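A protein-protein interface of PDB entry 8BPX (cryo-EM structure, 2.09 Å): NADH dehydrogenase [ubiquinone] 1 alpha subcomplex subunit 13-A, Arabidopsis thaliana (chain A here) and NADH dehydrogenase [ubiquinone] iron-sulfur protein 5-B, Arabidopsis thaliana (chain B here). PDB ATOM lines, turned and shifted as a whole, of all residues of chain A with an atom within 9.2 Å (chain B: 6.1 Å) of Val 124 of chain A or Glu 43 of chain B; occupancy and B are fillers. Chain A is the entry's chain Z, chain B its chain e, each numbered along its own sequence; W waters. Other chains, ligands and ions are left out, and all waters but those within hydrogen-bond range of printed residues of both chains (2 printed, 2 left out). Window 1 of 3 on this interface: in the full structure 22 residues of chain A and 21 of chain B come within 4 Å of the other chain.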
ATOM      1  N   TRP A 101      32.442  17.205  14.953  1.00  0.00           N
ATOM      2  CA  TRP A 101      31.192  17.601  14.320  1.00  0.00           C
ATOM      3  C   TRP A 101      29.990  17.059  15.081  1.00  0.00           C
ATOM      4  O   TRP A 101      28.970  17.744  15.200  1.00  0.00           O
ATOM      5  CB  TRP A 101      31.162  17.129  12.868  1.00  0.00           C
ATOM      6  CG  TRP A 101      29.992  17.667  12.121  1.00  0.00           C
ATOM      7  CD1 TRP A 101      28.933  16.960  11.632  1.00  0.00           C
ATOM      8  CD2 TRP A 101      29.750  19.035  11.789  1.00  0.00           C
ATOM      9  NE1 TRP A 101      28.048  17.805  11.011  1.00  0.00           N
ATOM     10  CE2 TRP A 101      28.528  19.085  11.092  1.00  0.00           C
ATOM     11  CE3 TRP A 101      30.451  20.226  12.010  1.00  0.00           C
ATOM     12  CZ2 TRP A 101      27.992  20.275  10.617  1.00  0.00           C
ATOM     13  CZ3 TRP A 101      29.916  21.406  11.534  1.00  0.00           C
ATOM     14  CH2 TRP A 101      28.697  21.422  10.847  1.00  0.00           C
ATOM     15  N   TRP A 118      13.682  25.145  13.040  1.00  0.00           N
ATOM     16  CA  TRP A 118      15.088  24.825  12.870  1.00  0.00           C
ATOM     17  C   TRP A 118      15.271  23.384  12.400  1.00  0.00           C
ATOM     18  O   TRP A 118      14.399  22.526  12.561  1.00  0.00           O
ATOM     19  CB  TRP A 118      15.853  25.049  14.175  1.00  0.00           C
ATOM     20  CG  TRP A 118      17.288  25.391  13.961  1.00  0.00           C
ATOM     21  CD1 TRP A 118      18.368  24.619  14.267  1.00  0.00           C
ATOM     22  CD2 TRP A 118      17.805  26.591  13.374  1.00  0.00           C
ATOM     23  NE1 TRP A 118      19.529  25.264  13.914  1.00  0.00           N
ATOM     24  CE2 TRP A 118      19.211  26.479  13.365  1.00  0.00           C
ATOM     25  CE3 TRP A 118      17.218  27.749  12.860  1.00  0.00           C
ATOM     26  CZ2 TRP A 118      20.036  27.481  12.860  1.00  0.00           C
ATOM     27  CZ3 TRP A 118      18.040  28.744  12.358  1.00  0.00           C
ATOM     28  CH2 TRP A 118      19.433  28.602  12.363  1.00  0.00           C
ATOM     29  N   LYS A 119      16.429  23.137  11.790  1.00  0.00           N
ATOM     30  CA  LYS A 119      16.873  21.798  11.422  1.00  0.00           C
ATOM     31  C   LYS A 119      18.354  21.705  11.741  1.00  0.00           C
ATOM     32  O   LYS A 119      19.161  22.427  11.148  1.00  0.00           O
ATOM     33  CB  LYS A 119      16.622  21.501   9.942  1.00  0.00           C
ATOM     34  CG  LYS A 119      15.182  21.194   9.597  1.00  0.00           C
ATOM     35  CD  LYS A 119      14.887  21.502   8.140  1.00  0.00           C
ATOM     36  CE  LYS A 119      13.500  21.025   7.749  1.00  0.00           C
ATOM     37  NZ  LYS A 119      13.426  19.539   7.705  1.00  0.00           N
ATOM     38  N   GLY A 121      22.092  21.017  11.868  1.00  0.00           N
ATOM     39  CA  GLY A 121      23.063  20.642  10.852  1.00  0.00           C
ATOM     40  C   GLY A 121      22.503  20.611   9.446  1.00  0.00           C
ATOM     41  O   GLY A 121      22.823  19.700   8.674  1.00  0.00           O
ATOM     42  N   GLU A 122      21.672  21.587   9.095  1.00  0.00           N
ATOM     43  CA  GLU A 122      21.108  21.636   7.754  1.00  0.00           C
ATOM     44  C   GLU A 122      22.182  22.033   6.746  1.00  0.00           C
ATOM     45  O   GLU A 122      22.926  22.992   6.961  1.00  0.00           O
ATOM     46  CB  GLU A 122      19.936  22.618   7.708  1.00  0.00           C
ATOM     47  CG  GLU A 122      19.491  22.991   6.309  1.00  0.00           C
ATOM     48  CD  GLU A 122      18.038  23.428   6.245  1.00  0.00           C
ATOM     49  OE1 GLU A 122      17.237  22.726   5.595  1.00  0.00           O
ATOM     50  OE2 GLU A 122      17.699  24.474   6.838  1.00  0.00           O
ATOM     51  N   ASN A 123      22.264  21.287   5.646  1.00  0.00           N
ATOM     52  CA  ASN A 123      23.191  21.619   4.571  1.00  0.00           C
ATOM     53  C   ASN A 123      22.657  22.811   3.784  1.00  0.00           C
ATOM     54  O   ASN A 123      21.540  22.765   3.260  1.00  0.00           O
ATOM     55  CB  ASN A 123      23.387  20.414   3.655  1.00  0.00           C
ATOM     56  CG  ASN A 123      24.603  20.547   2.753  1.00  0.00           C
ATOM     57  OD1 ASN A 123      25.096  21.647   2.504  1.00  0.00           O
ATOM     58  ND2 ASN A 123      25.087  19.420   2.254  1.00  0.00           N
ATOM     59  N   VAL A 124      23.450  23.880   3.698  1.00  0.00           N
ATOM     60  CA  VAL A 124      22.990  25.062   2.975  1.00  0.00           C
ATOM     61  C   VAL A 124      23.114  24.898   1.464  1.00  0.00           C
ATOM     62  O   VAL A 124      22.509  25.675   0.717  1.00  0.00           O
ATOM     63  CB  VAL A 124      23.740  26.327   3.428  1.00  0.00           C
ATOM     64  CG1 VAL A 124      23.424  26.644   4.888  1.00  0.00           C
ATOM     65  CG2 VAL A 124      25.237  26.183   3.202  1.00  0.00           C
ATOM     66  N   TYR A 125      23.877  23.916   0.993  1.00  0.00           N
ATOM     67  CA  TYR A 125      23.995  23.662  -0.436  1.00  0.00           C
ATOM     68  C   TYR A 125      22.841  22.788  -0.909  1.00  0.00           C
ATOM     69  O   TYR A 125      22.543  21.755  -0.301  1.00  0.00           O
ATOM     70  CB  TYR A 125      25.335  22.998  -0.748  1.00  0.00           C
ATOM     71  CG  TYR A 125      26.513  23.921  -0.538  1.00  0.00           C
ATOM     72  CD1 TYR A 125      26.781  24.945  -1.436  1.00  0.00           C
ATOM     73  CD2 TYR A 125      27.343  23.785   0.569  1.00  0.00           C
ATOM     74  CE1 TYR A 125      27.843  25.800  -1.249  1.00  0.00           C
ATOM     75  CE2 TYR A 125      28.414  24.636   0.764  1.00  0.00           C
ATOM     76  CZ  TYR A 125      28.657  25.643  -0.151  1.00  0.00           C
ATOM     77  OH  TYR A 125      29.715  26.497   0.032  1.00  0.00           O
ATOM     78  N   ASN A 126      22.184  23.212  -1.993  1.00  0.00           N
ATOM     79  CA  ASN A 126      21.061  22.449  -2.531  1.00  0.00           C
ATOM     80  C   ASN A 126      21.507  21.079  -3.025  1.00  0.00           C
ATOM     81  O   ASN A 126      20.812  20.080  -2.812  1.00  0.00           O
ATOM     82  CB  ASN A 126      20.389  23.226  -3.656  1.00  0.00           C
ATOM     83  CG  ASN A 126      19.899  24.581  -3.209  1.00  0.00           C
ATOM     84  OD1 ASN A 126      20.398  25.609  -3.653  1.00  0.00           O
ATOM     85  ND2 ASN A 126      18.919  24.589  -2.320  1.00  0.00           N
ATOM     86  N   SER A 127      22.665  21.012  -3.683  1.00  0.00           N
ATOM     87  CA  SER A 127      23.165  19.736  -4.175  1.00  0.00           C
ATOM     88  C   SER A 127      23.407  18.739  -3.052  1.00  0.00           C
ATOM     89  O   SER A 127      23.465  17.534  -3.310  1.00  0.00           O
ATOM     90  CB  SER A 127      24.456  19.949  -4.966  1.00  0.00           C
ATOM     91  OG  SER A 127      25.588  19.881  -4.118  1.00  0.00           O
ATOM     92  N   GLY A 128      23.551  19.213  -1.815  1.00  0.00           N
ATOM     93  CA  GLY A 128      23.803  18.347  -0.687  1.00  0.00           C
ATOM     94  C   GLY A 128      25.197  17.771  -0.624  1.00  0.00           C
ATOM     95  O   GLY A 128      25.495  17.019   0.309  1.00  0.00           O
ATOM     96  N   ARG A 129      26.062  18.100  -1.577  1.00  0.00           N
ATOM     97  CA  ARG A 129      27.424  17.596  -1.534  1.00  0.00           C
ATOM     98  C   ARG A 129      28.176  18.221  -0.365  1.00  0.00           C
ATOM     99  O   ARG A 129      27.937  19.370   0.019  1.00  0.00           O
ATOM    100  CB  ARG A 129      28.127  17.857  -2.868  1.00  0.00           C
ATOM    101  CG  ARG A 129      29.549  18.365  -2.781  1.00  0.00           C
ATOM    102  CD  ARG A 129      30.141  18.496  -4.175  1.00  0.00           C
ATOM    103  NE  ARG A 129      29.623  19.626  -4.935  1.00  0.00           N
ATOM    104  CZ  ARG A 129      29.845  19.812  -6.232  1.00  0.00           C
ATOM    105  NH1 ARG A 129      30.561  18.954  -6.938  1.00  0.00           N
ATOM    106  NH2 ARG A 129      29.345  20.888  -6.829  1.00  0.00           N
ATOM    107  N   TRP A 130      29.067  17.436   0.225  1.00  0.00           N
ATOM    108  CA  TRP A 130      29.707  17.821   1.472  1.00  0.00           C
ATOM    109  C   TRP A 130      30.801  18.849   1.223  1.00  0.00           C
ATOM    110  O   TRP A 130      31.630  18.685   0.326  1.00  0.00           O
ATOM    111  CB  TRP A 130      30.286  16.594   2.171  1.00  0.00           C
ATOM    112  CG  TRP A 130      30.807  16.906   3.525  1.00  0.00           C
ATOM    113  CD1 TRP A 130      30.094  16.956   4.685  1.00  0.00           C
ATOM    114  CD2 TRP A 130      32.156  17.233   3.868  1.00  0.00           C
ATOM    115  NE1 TRP A 130      30.917  17.287   5.730  1.00  0.00           N
ATOM    116  CE2 TRP A 130      32.190  17.460   5.256  1.00  0.00           C
ATOM    117  CE3 TRP A 130      33.342  17.347   3.135  1.00  0.00           C
ATOM    118  CZ2 TRP A 130      33.361  17.797   5.927  1.00  0.00           C
ATOM    119  CZ3 TRP A 130      34.503  17.681   3.803  1.00  0.00           C
ATOM    120  CH2 TRP A 130      34.504  17.904   5.184  1.00  0.00           C
ATOM    121  N   MET A 131      30.799  19.907   2.027  1.00  0.00           N
ATOM    122  CA  MET A 131      31.858  20.900   2.051  1.00  0.00           C
ATOM    123  C   MET A 131      32.314  21.102   3.488  1.00  0.00           C
ATOM    124  O   MET A 131      31.504  21.023   4.415  1.00  0.00           O
ATOM    125  CB  MET A 131      31.388  22.242   1.468  1.00  0.00           C
ATOM    126  CG  MET A 131      30.936  22.173   0.012  1.00  0.00           C
ATOM    127  SD  MET A 131      32.286  22.030  -1.174  1.00  0.00           S
ATOM    128  CE  MET A 131      33.249  23.490  -0.791  1.00  0.00           C
ATOM    129  N   PRO A 132      33.604  21.354   3.703  1.00  0.00           N
ATOM    130  CA  PRO A 132      34.068  21.652   5.054  1.00  0.00           C
ATOM    131  C   PRO A 132      33.445  22.938   5.553  1.00  0.00           C
ATOM    132  O   PRO A 132      33.083  23.825   4.756  1.00  0.00           O
ATOM    133  CB  PRO A 132      35.590  21.788   4.889  1.00  0.00           C
ATOM    134  CG  PRO A 132      35.919  21.334   3.519  1.00  0.00           C
ATOM    135  CD  PRO A 132      34.681  21.377   2.700  1.00  0.00           C
ATOM    136  N   PRO A 133      33.282  23.082   6.866  1.00  0.00           N
ATOM    137  CA  PRO A 133      32.698  24.321   7.396  1.00  0.00           C
ATOM    138  C   PRO A 133      33.578  25.522   7.075  1.00  0.00           C
ATOM    139  O   PRO A 133      34.799  25.487   7.251  1.00  0.00           O
ATOM    140  CB  PRO A 133      32.612  24.065   8.906  1.00  0.00           C
ATOM    141  CG  PRO A 133      32.888  22.605   9.096  1.00  0.00           C
ATOM    142  CD  PRO A 133      33.719  22.173   7.936  1.00  0.00           C
ATOM    143  N   ALA A 134      32.947  26.584   6.588  1.00  0.00           N
ATOM    144  CA  ALA A 134      33.670  27.809   6.286  1.00  0.00           C
ATOM    145  C   ALA A 134      34.119  28.478   7.580  1.00  0.00           C
ATOM    146  O   ALA A 134      33.444  28.411   8.609  1.00  0.00           O
ATOM    147  CB  ALA A 134      32.796  28.755   5.463  1.00  0.00           C
ATOM    148  N   CYS B  14      35.484  26.460  -5.727  1.00  0.00           N
ATOM    149  CA  CYS B  14      34.123  26.612  -6.282  1.00  0.00           C
ATOM    150  C   CYS B  14      33.968  26.212  -7.772  1.00  0.00           C
ATOM    151  O   CYS B  14      32.931  26.384  -8.282  1.00  0.00           O
ATOM    152  CB  CYS B  14      33.704  28.059  -6.075  1.00  0.00           C
ATOM    153  SG  CYS B  14      33.776  28.564  -4.343  1.00  0.00           S
ATOM    154  N   ARG B  38      23.010  27.656  -9.446  1.00  0.00           N
ATOM    155  CA  ARG B  38      23.591  28.994  -9.414  1.00  0.00           C
ATOM    156  C   ARG B  38      23.768  29.492  -7.986  1.00  0.00           C
ATOM    157  O   ARG B  38      24.814  30.060  -7.636  1.00  0.00           O
ATOM    158  CB  ARG B  38      22.713  29.957 -10.204  1.00  0.00           C
ATOM    159  CG  ARG B  38      23.268  31.358 -10.315  1.00  0.00           C
ATOM    160  CD  ARG B  38      22.146  32.339 -10.530  1.00  0.00           C
ATOM    161  NE  ARG B  38      22.607  33.668 -10.908  1.00  0.00           N
ATOM    162  CZ  ARG B  38      22.526  34.734 -10.124  1.00  0.00           C
ATOM    163  NH1 ARG B  38      22.007  34.660  -8.909  1.00  0.00           N
ATOM    164  NH2 ARG B  38      22.974  35.902 -10.570  1.00  0.00           N
ATOM    165  N   GLU B  39      22.750  29.303  -7.143  1.00  0.00           N
ATOM    166  CA  GLU B  39      22.878  29.762  -5.768  1.00  0.00           C
ATOM    167  C   GLU B  39      23.859  28.899  -4.988  1.00  0.00           C
ATOM    168  O   GLU B  39      24.499  29.392  -4.059  1.00  0.00           O
ATOM    169  CB  GLU B  39      21.507  29.820  -5.088  1.00  0.00           C
ATOM    170  CG  GLU B  39      20.879  28.496  -4.750  1.00  0.00           C
ATOM    171  CD  GLU B  39      19.378  28.615  -4.561  1.00  0.00           C
ATOM    172  OE1 GLU B  39      18.780  29.530  -5.160  1.00  0.00           O
ATOM    173  OE2 GLU B  39      18.800  27.810  -3.804  1.00  0.00           O
ATOM    174  N   ASP B  40      24.035  27.633  -5.379  1.00  0.00           N
ATOM    175  CA  ASP B  40      25.106  26.834  -4.790  1.00  0.00           C
ATOM    176  C   ASP B  40      26.481  27.404  -5.135  1.00  0.00           C
ATOM    177  O   ASP B  40      27.361  27.495  -4.270  1.00  0.00           O
ATOM    178  CB  ASP B  40      24.995  25.383  -5.252  1.00  0.00           C
ATOM    179  CG  ASP B  40      24.155  24.535  -4.313  1.00  0.00           C
ATOM    180  OD1 ASP B  40      23.445  25.117  -3.466  1.00  0.00           O
ATOM    181  OD2 ASP B  40      24.197  23.295  -4.427  1.00  0.00           O
ATOM    182  N   TYR B  41      26.743  27.719  -6.400  1.00  0.00           N
ATOM    183  CA  TYR B  41      28.001  28.406  -6.831  1.00  0.00           C
ATOM    184  C   TYR B  41      28.220  29.700  -6.020  1.00  0.00           C
ATOM    185  O   TYR B  41      29.243  29.797  -5.421  1.00  0.00           O
ATOM    186  CB  TYR B  41      28.000  28.613  -8.350  1.00  0.00           C
ATOM    187  CG  TYR B  41      29.135  29.501  -8.807  1.00  0.00           C
ATOM    188  CD1 TYR B  41      30.440  29.054  -8.757  1.00  0.00           C
ATOM    189  CD2 TYR B  41      28.912  30.806  -9.213  1.00  0.00           C
ATOM    190  CE1 TYR B  41      31.496  29.857  -9.151  1.00  0.00           C
ATOM    191  CE2 TYR B  41      29.952  31.632  -9.610  1.00  0.00           C
ATOM    192  CZ  TYR B  41      31.252  31.151  -9.576  1.00  0.00           C
ATOM    193  OH  TYR B  41      32.299  31.925  -9.956  1.00  0.00           O
ATOM    194  N   LEU B  42      27.211  30.561  -5.944  1.00  0.00           N
ATOM    195  CA  LEU B  42      27.402  31.826  -5.239  1.00  0.00           C
ATOM    196  C   LEU B  42      27.585  31.620  -3.735  1.00  0.00           C
ATOM    197  O   LEU B  42      28.338  32.368  -3.095  1.00  0.00           O
ATOM    198  CB  LEU B  42      26.237  32.769  -5.529  1.00  0.00           C
ATOM    199  CG  LEU B  42      26.103  33.195  -6.998  1.00  0.00           C
ATOM    200  CD1 LEU B  42      24.920  34.126  -7.193  1.00  0.00           C
ATOM    201  CD2 LEU B  42      27.383  33.844  -7.514  1.00  0.00           C
ATOM    202  N   GLU B  43      26.923  30.610  -3.159  1.00  0.00           N
ATOM    203  CA  GLU B  43      27.148  30.260  -1.761  1.00  0.00           C
ATOM    204  C   GLU B  43      28.579  29.796  -1.533  1.00  0.00           C
ATOM    205  O   GLU B  43      29.194  30.136  -0.517  1.00  0.00           O
ATOM    206  CB  GLU B  43      26.160  29.173  -1.334  1.00  0.00           C
ATOM    207  CG  GLU B  43      26.297  28.685   0.109  1.00  0.00           C
ATOM    208  CD  GLU B  43      26.121  29.785   1.148  1.00  0.00           C
ATOM    209  OE1 GLU B  43      25.383  30.755   0.888  1.00  0.00           O
ATOM    210  OE2 GLU B  43      26.714  29.669   2.238  1.00  0.00           O
ATOM    211  N   CYS B  44      29.121  29.002  -2.458  1.00  0.00           N
ATOM    212  CA  CYS B  44      30.527  28.634  -2.353  1.00  0.00           C
ATOM    213  C   CYS B  44      31.418  29.868  -2.420  1.00  0.00           C
ATOM    214  O   CYS B  44      32.430  29.951  -1.714  1.00  0.00           O
ATOM    215  CB  CYS B  44      30.907  27.640  -3.449  1.00  0.00           C
ATOM    216  SG  CYS B  44      32.624  27.075  -3.378  1.00  0.00           S
ATOM    217  N   LEU B  45      31.116  30.885  -3.163  1.00  0.00           N
ATOM    218  CA  LEU B  45      32.000  32.082  -3.266  1.00  0.00           C
ATOM    219  C   LEU B  45      31.928  32.879  -1.968  1.00  0.00           C
ATOM    220  O   LEU B  45      32.949  33.259  -1.496  1.00  0.00           O
ATOM    221  CB  LEU B  45      31.558  33.043  -4.360  1.00  0.00           C
ATOM    222  CG  LEU B  45      31.624  32.569  -5.813  1.00  0.00           C
ATOM    223  CD1 LEU B  45      31.270  33.710  -6.749  1.00  0.00           C
ATOM    224  CD2 LEU B  45      32.974  31.996  -6.178  1.00  0.00           C
ATOM    225  N   HIS B  46      30.707  33.062  -1.457  1.00  0.00           N
ATOM    226  CA  HIS B  46      30.623  34.017  -0.355  1.00  0.00           C
ATOM    227  C   HIS B  46      30.181  33.445   0.989  1.00  0.00           C
ATOM    228  O   HIS B  46      30.280  34.160   1.992  1.00  0.00           O
ATOM    229  CB  HIS B  46      29.688  35.178  -0.725  1.00  0.00           C
ATOM    230  CG  HIS B  46      29.888  35.699  -2.113  1.00  0.00           C
ATOM    231  ND1 HIS B  46      31.009  36.407  -2.488  1.00  0.00           N
ATOM    232  CD2 HIS B  46      29.104  35.624  -3.215  1.00  0.00           C
ATOM    233  CE1 HIS B  46      30.911  36.740  -3.762  1.00  0.00           C
ATOM    234  NE2 HIS B  46      29.765  36.277  -4.227  1.00  0.00           N
ATOM    235  N   HIS B  47      29.698  32.202   1.048  1.00  0.00           N
ATOM    236  CA  HIS B  47      29.257  31.576   2.302  1.00  0.00           C
ATOM    237  C   HIS B  47      28.201  32.408   3.027  1.00  0.00           C
ATOM    238  O   HIS B  47      28.168  32.440   4.258  1.00  0.00           O
ATOM    239  CB  HIS B  47      30.431  31.306   3.249  1.00  0.00           C
ATOM    240  CG  HIS B  47      31.634  30.719   2.583  1.00  0.00           C
ATOM    241  ND1 HIS B  47      31.640  29.455   2.034  1.00  0.00           N
ATOM    242  CD2 HIS B  47      32.879  31.217   2.392  1.00  0.00           C
ATOM    243  CE1 HIS B  47      32.833  29.203   1.529  1.00  0.00           C
ATOM    244  NE2 HIS B  47      33.603  30.256   1.732  1.00  0.00           N
ATOM    245  N   SER B  48      27.330  33.087   2.281  1.00  0.00           N
ATOM    246  CA  SER B  48      26.405  34.025   2.904  1.00  0.00           C
ATOM    247  C   SER B  48      25.385  33.308   3.785  1.00  0.00           C
ATOM    248  O   SER B  48      25.175  33.687   4.943  1.00  0.00           O
ATOM    249  CB  SER B  48      25.707  34.861   1.831  1.00  0.00           C
ATOM    250  OG  SER B  48      24.447  35.323   2.280  1.00  0.00           O
ATOM    251  N   LYS B  49      24.748  32.259   3.261  1.00  0.00           N
ATOM    252  CA  LYS B  49      23.714  31.576   4.035  1.00  0.00           C
ATOM    253  C   LYS B  49      24.307  30.801   5.206  1.00  0.00           C
ATOM    254  O   LYS B  49      23.715  30.763   6.293  1.00  0.00           O
ATOM    255  CB  LYS B  49      22.887  30.663   3.131  1.00  0.00           C
ATOM    256  CG  LYS B  49      22.054  31.420   2.109  1.00  0.00           C
ATOM    257  CD  LYS B  49      21.408  30.510   1.071  1.00  0.00           C
ATOM    258  CE  LYS B  49      22.290  29.357   0.669  1.00  0.00           C
ATOM    259  NZ  LYS B  49      23.232  29.775  -0.391  1.00  0.00           N
ATOM    260  N   GLU B  50      25.472  30.185   5.005  1.00  0.00           N
ATOM    261  CA  GLU B  50      26.155  29.488   6.092  1.00  0.00           C
ATOM    262  C   GLU B  50      26.425  30.427   7.262  1.00  0.00           C
ATOM    263  O   GLU B  50      26.078  30.129   8.415  1.00  0.00           O
ATOM    264  CB  GLU B  50      27.465  28.892   5.572  1.00  0.00           C
ATOM    265  CG  GLU B  50      27.918  27.620   6.269  1.00  0.00           C
ATOM    266  CD  GLU B  50      29.380  27.298   6.007  1.00  0.00           C
ATOM    267  OE1 GLU B  50      29.737  27.038   4.838  1.00  0.00           O
ATOM    268  OE2 GLU B  50      30.172  27.282   6.969  1.00  0.00           O
ATOM    269  N   PHE B  51      27.034  31.577   6.975  1.00  0.00           N
ATOM    270  CA  PHE B  51      27.371  32.527   8.026  1.00  0.00           C
ATOM    271  C   PHE B  51      26.116  33.132   8.644  1.00  0.00           C
ATOM    272  O   PHE B  51      26.079  33.386   9.850  1.00  0.00           O
ATOM    273  CB  PHE B  51      28.296  33.614   7.473  1.00  0.00           C
ATOM    274  CG  PHE B  51      29.677  33.118   7.129  1.00  0.00           C
ATOM    275  CD1 PHE B  51      30.095  31.861   7.530  1.00  0.00           C
ATOM    276  CD2 PHE B  51      30.558  33.908   6.410  1.00  0.00           C
ATOM    277  CE1 PHE B  51      31.354  31.399   7.219  1.00  0.00           C
ATOM    278  CE2 PHE B  51      31.824  33.451   6.094  1.00  0.00           C
ATOM    279  CZ  PHE B  51      32.224  32.198   6.497  1.00  0.00           C
ATOM    280  N   ARG B  53      23.197  31.598   9.045  1.00  0.00           N
ATOM    281  CA  ARG B  53      22.653  30.588   9.950  1.00  0.00           C
ATOM    282  C   ARG B  53      23.482  30.484  11.229  1.00  0.00           C
ATOM    283  O   ARG B  53      22.936  30.401  12.342  1.00  0.00           O
ATOM    284  CB  ARG B  53      22.586  29.246   9.222  1.00  0.00           C
ATOM    285  CG  ARG B  53      22.601  28.022  10.113  1.00  0.00           C
ATOM    286  CD  ARG B  53      22.562  26.759   9.273  1.00  0.00           C
ATOM    287  NE  ARG B  53      22.360  25.567  10.085  1.00  0.00           N
ATOM    288  CZ  ARG B  53      21.171  25.044  10.355  1.00  0.00           C
ATOM    289  NH1 ARG B  53      20.058  25.594   9.898  1.00  0.00           N
ATOM    290  NH2 ARG B  53      21.101  23.947  11.101  1.00  0.00           N
HETATM  291  O   HOH W   1      28.975  28.223   2.485  1.00  0.00           O
HETATM  292  O   HOH W   2      31.104  24.933   3.420  1.00  0.00           O
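Of the 16 printed residues of chain B, 9 touch a printed residue of chain A. Printed residues of chain A that touch a printed residue of chain B: Trp 118, Lys 119, Gly 121, Glu 122, Val 124, Tyr 125, Asn 126, Ser 127, Pro 133 and Ala 134. Hydrophobic or aromatic side chains of chain A that line the printed part of chain B: Trp 118, Val 124, Tyr 125 and Ala 134.
Among the printed residues, merely in contact across the chains: Val 124 of chain A with Glu 43 of chain B, Val 124 of chain A with Lys 49 of chain B, Tyr 125 of chain A with Asp 40 of chain B, Tyr 125 of chain A with Glu 43 of chain B, Tyr 125 of chain A with Cys 44 of chain B, Pro 133 of chain A with Glu 50 of chain B, Ala 134 of chain A with His 47 of chain B and Ala 134 of chain A with Phe 51 of chain B.
N of Tyr 125 of chain A lies within hydrogen-bond range of OD1 of Asn 123 of chain A, 3.0 Å away. OG of Ser 127 of chain A sits close to N of Arg 129 of chain A, at 3.1 Å. The side-chain sulfur (SG) of Cys 14 of chain B forms a disulfide with the side-chain sulfur (SG) of Cys 44 of chain B (2.1 Å). The backbone NH of Ser 48 of chain B is in hydrogen-bond range of the side-chain carboxylate of Glu 43 of chain B, at 3.3 Å. OE1 of Glu 43 of chain B lies within salt-bridge range of NZ of Lys 49 of chain B. The side-chain carboxylate of Glu 43 of chain B lies within hydrogen-bond range of the backbone NH of Glu 50 of chain B, at 3.1 Å.
Of chain B, only Glu 43 and Lys 49 come within 4 Å of Val 124 of chain A. Of chain A, only Val 124 (3.9 Å) and Tyr 125 (3.5 Å) come within 4 Å of Glu 43 of chain B. Of chain A, only Ala 134 comes within 4 Å of His 47 of chain B. No residue of chain A comes within 4 Å of Ser 48 of chain B. Lys 49 of chain B touches just one residue of chain A: Val 124. Of the printed residues of chain B, Gly 121 of chain A touches Arg 53. Of the printed residues of chain B, Asn 126 of chain A touches Glu 39 and Asp 40. The nearest residue of chain B that does not touch Val 124 of chain A is Glu 50 of chain B (4.1 Å). The nearest residue of chain A that does not touch Glu 43 of chain B is Ala 134 of chain A (6.9 Å). The nearest printed residue of chain B that does not touch Pro 133 of chain A is Phe 51 of chain B (6.3 Å).
Water W2 bridges the backbone carbonyl oxygen of Pro 132 of chain A (2.6 Å) and the side-chain carboxylate of Glu 50 of chain B (2.9 Å). Water W1 lies within hydrogen-bond range of the side-chain carboxylate of Glu 43 of chain B (2.7 Å), the side-chain carboxylate of Glu 50 of chain B (2.7 Å), a ring nitrogen (ND1) of His 47 of chain B (3.0 Å) and the side-chain hydroxyl of Tyr 125 of chain A (3.1 Å).
The guanidinium group (NH2) of Arg 53 of chain B lies within hydrogen-bond range of the backbone carbonyl oxygen (O) of Lys 119 of chain A, 2.5 Å away. OE2 of Glu 39 of chain B lies close to OD1 of Asn 126 of chain A (2.7 Å). The backbone NH (N) of Asn 126 of chain A sits at hydrogen-bond distance from the side-chain carboxylate (OD1) of Asp 40 of chain B (2.7 Å). N of Ser 127 of chain A lies within hydrogen-bond range of OD2 of Asp 40 of chain B (2.8 Å). N of Ala 134 of chain A lies within hydrogen-bond range of OE2 of Glu 50 of chain B (2.9 Å). NH2 of Arg 53 of chain B lies close to NE1 of Trp 118 of chain A, at 3.5 Å. N of Gly 121 of chain A sits close to NH2 of Arg 53 of chain B. The backbone NH of Glu 122 of chain A sits close to the guanidinium group of Arg 53 of chain B (3.1 Å).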
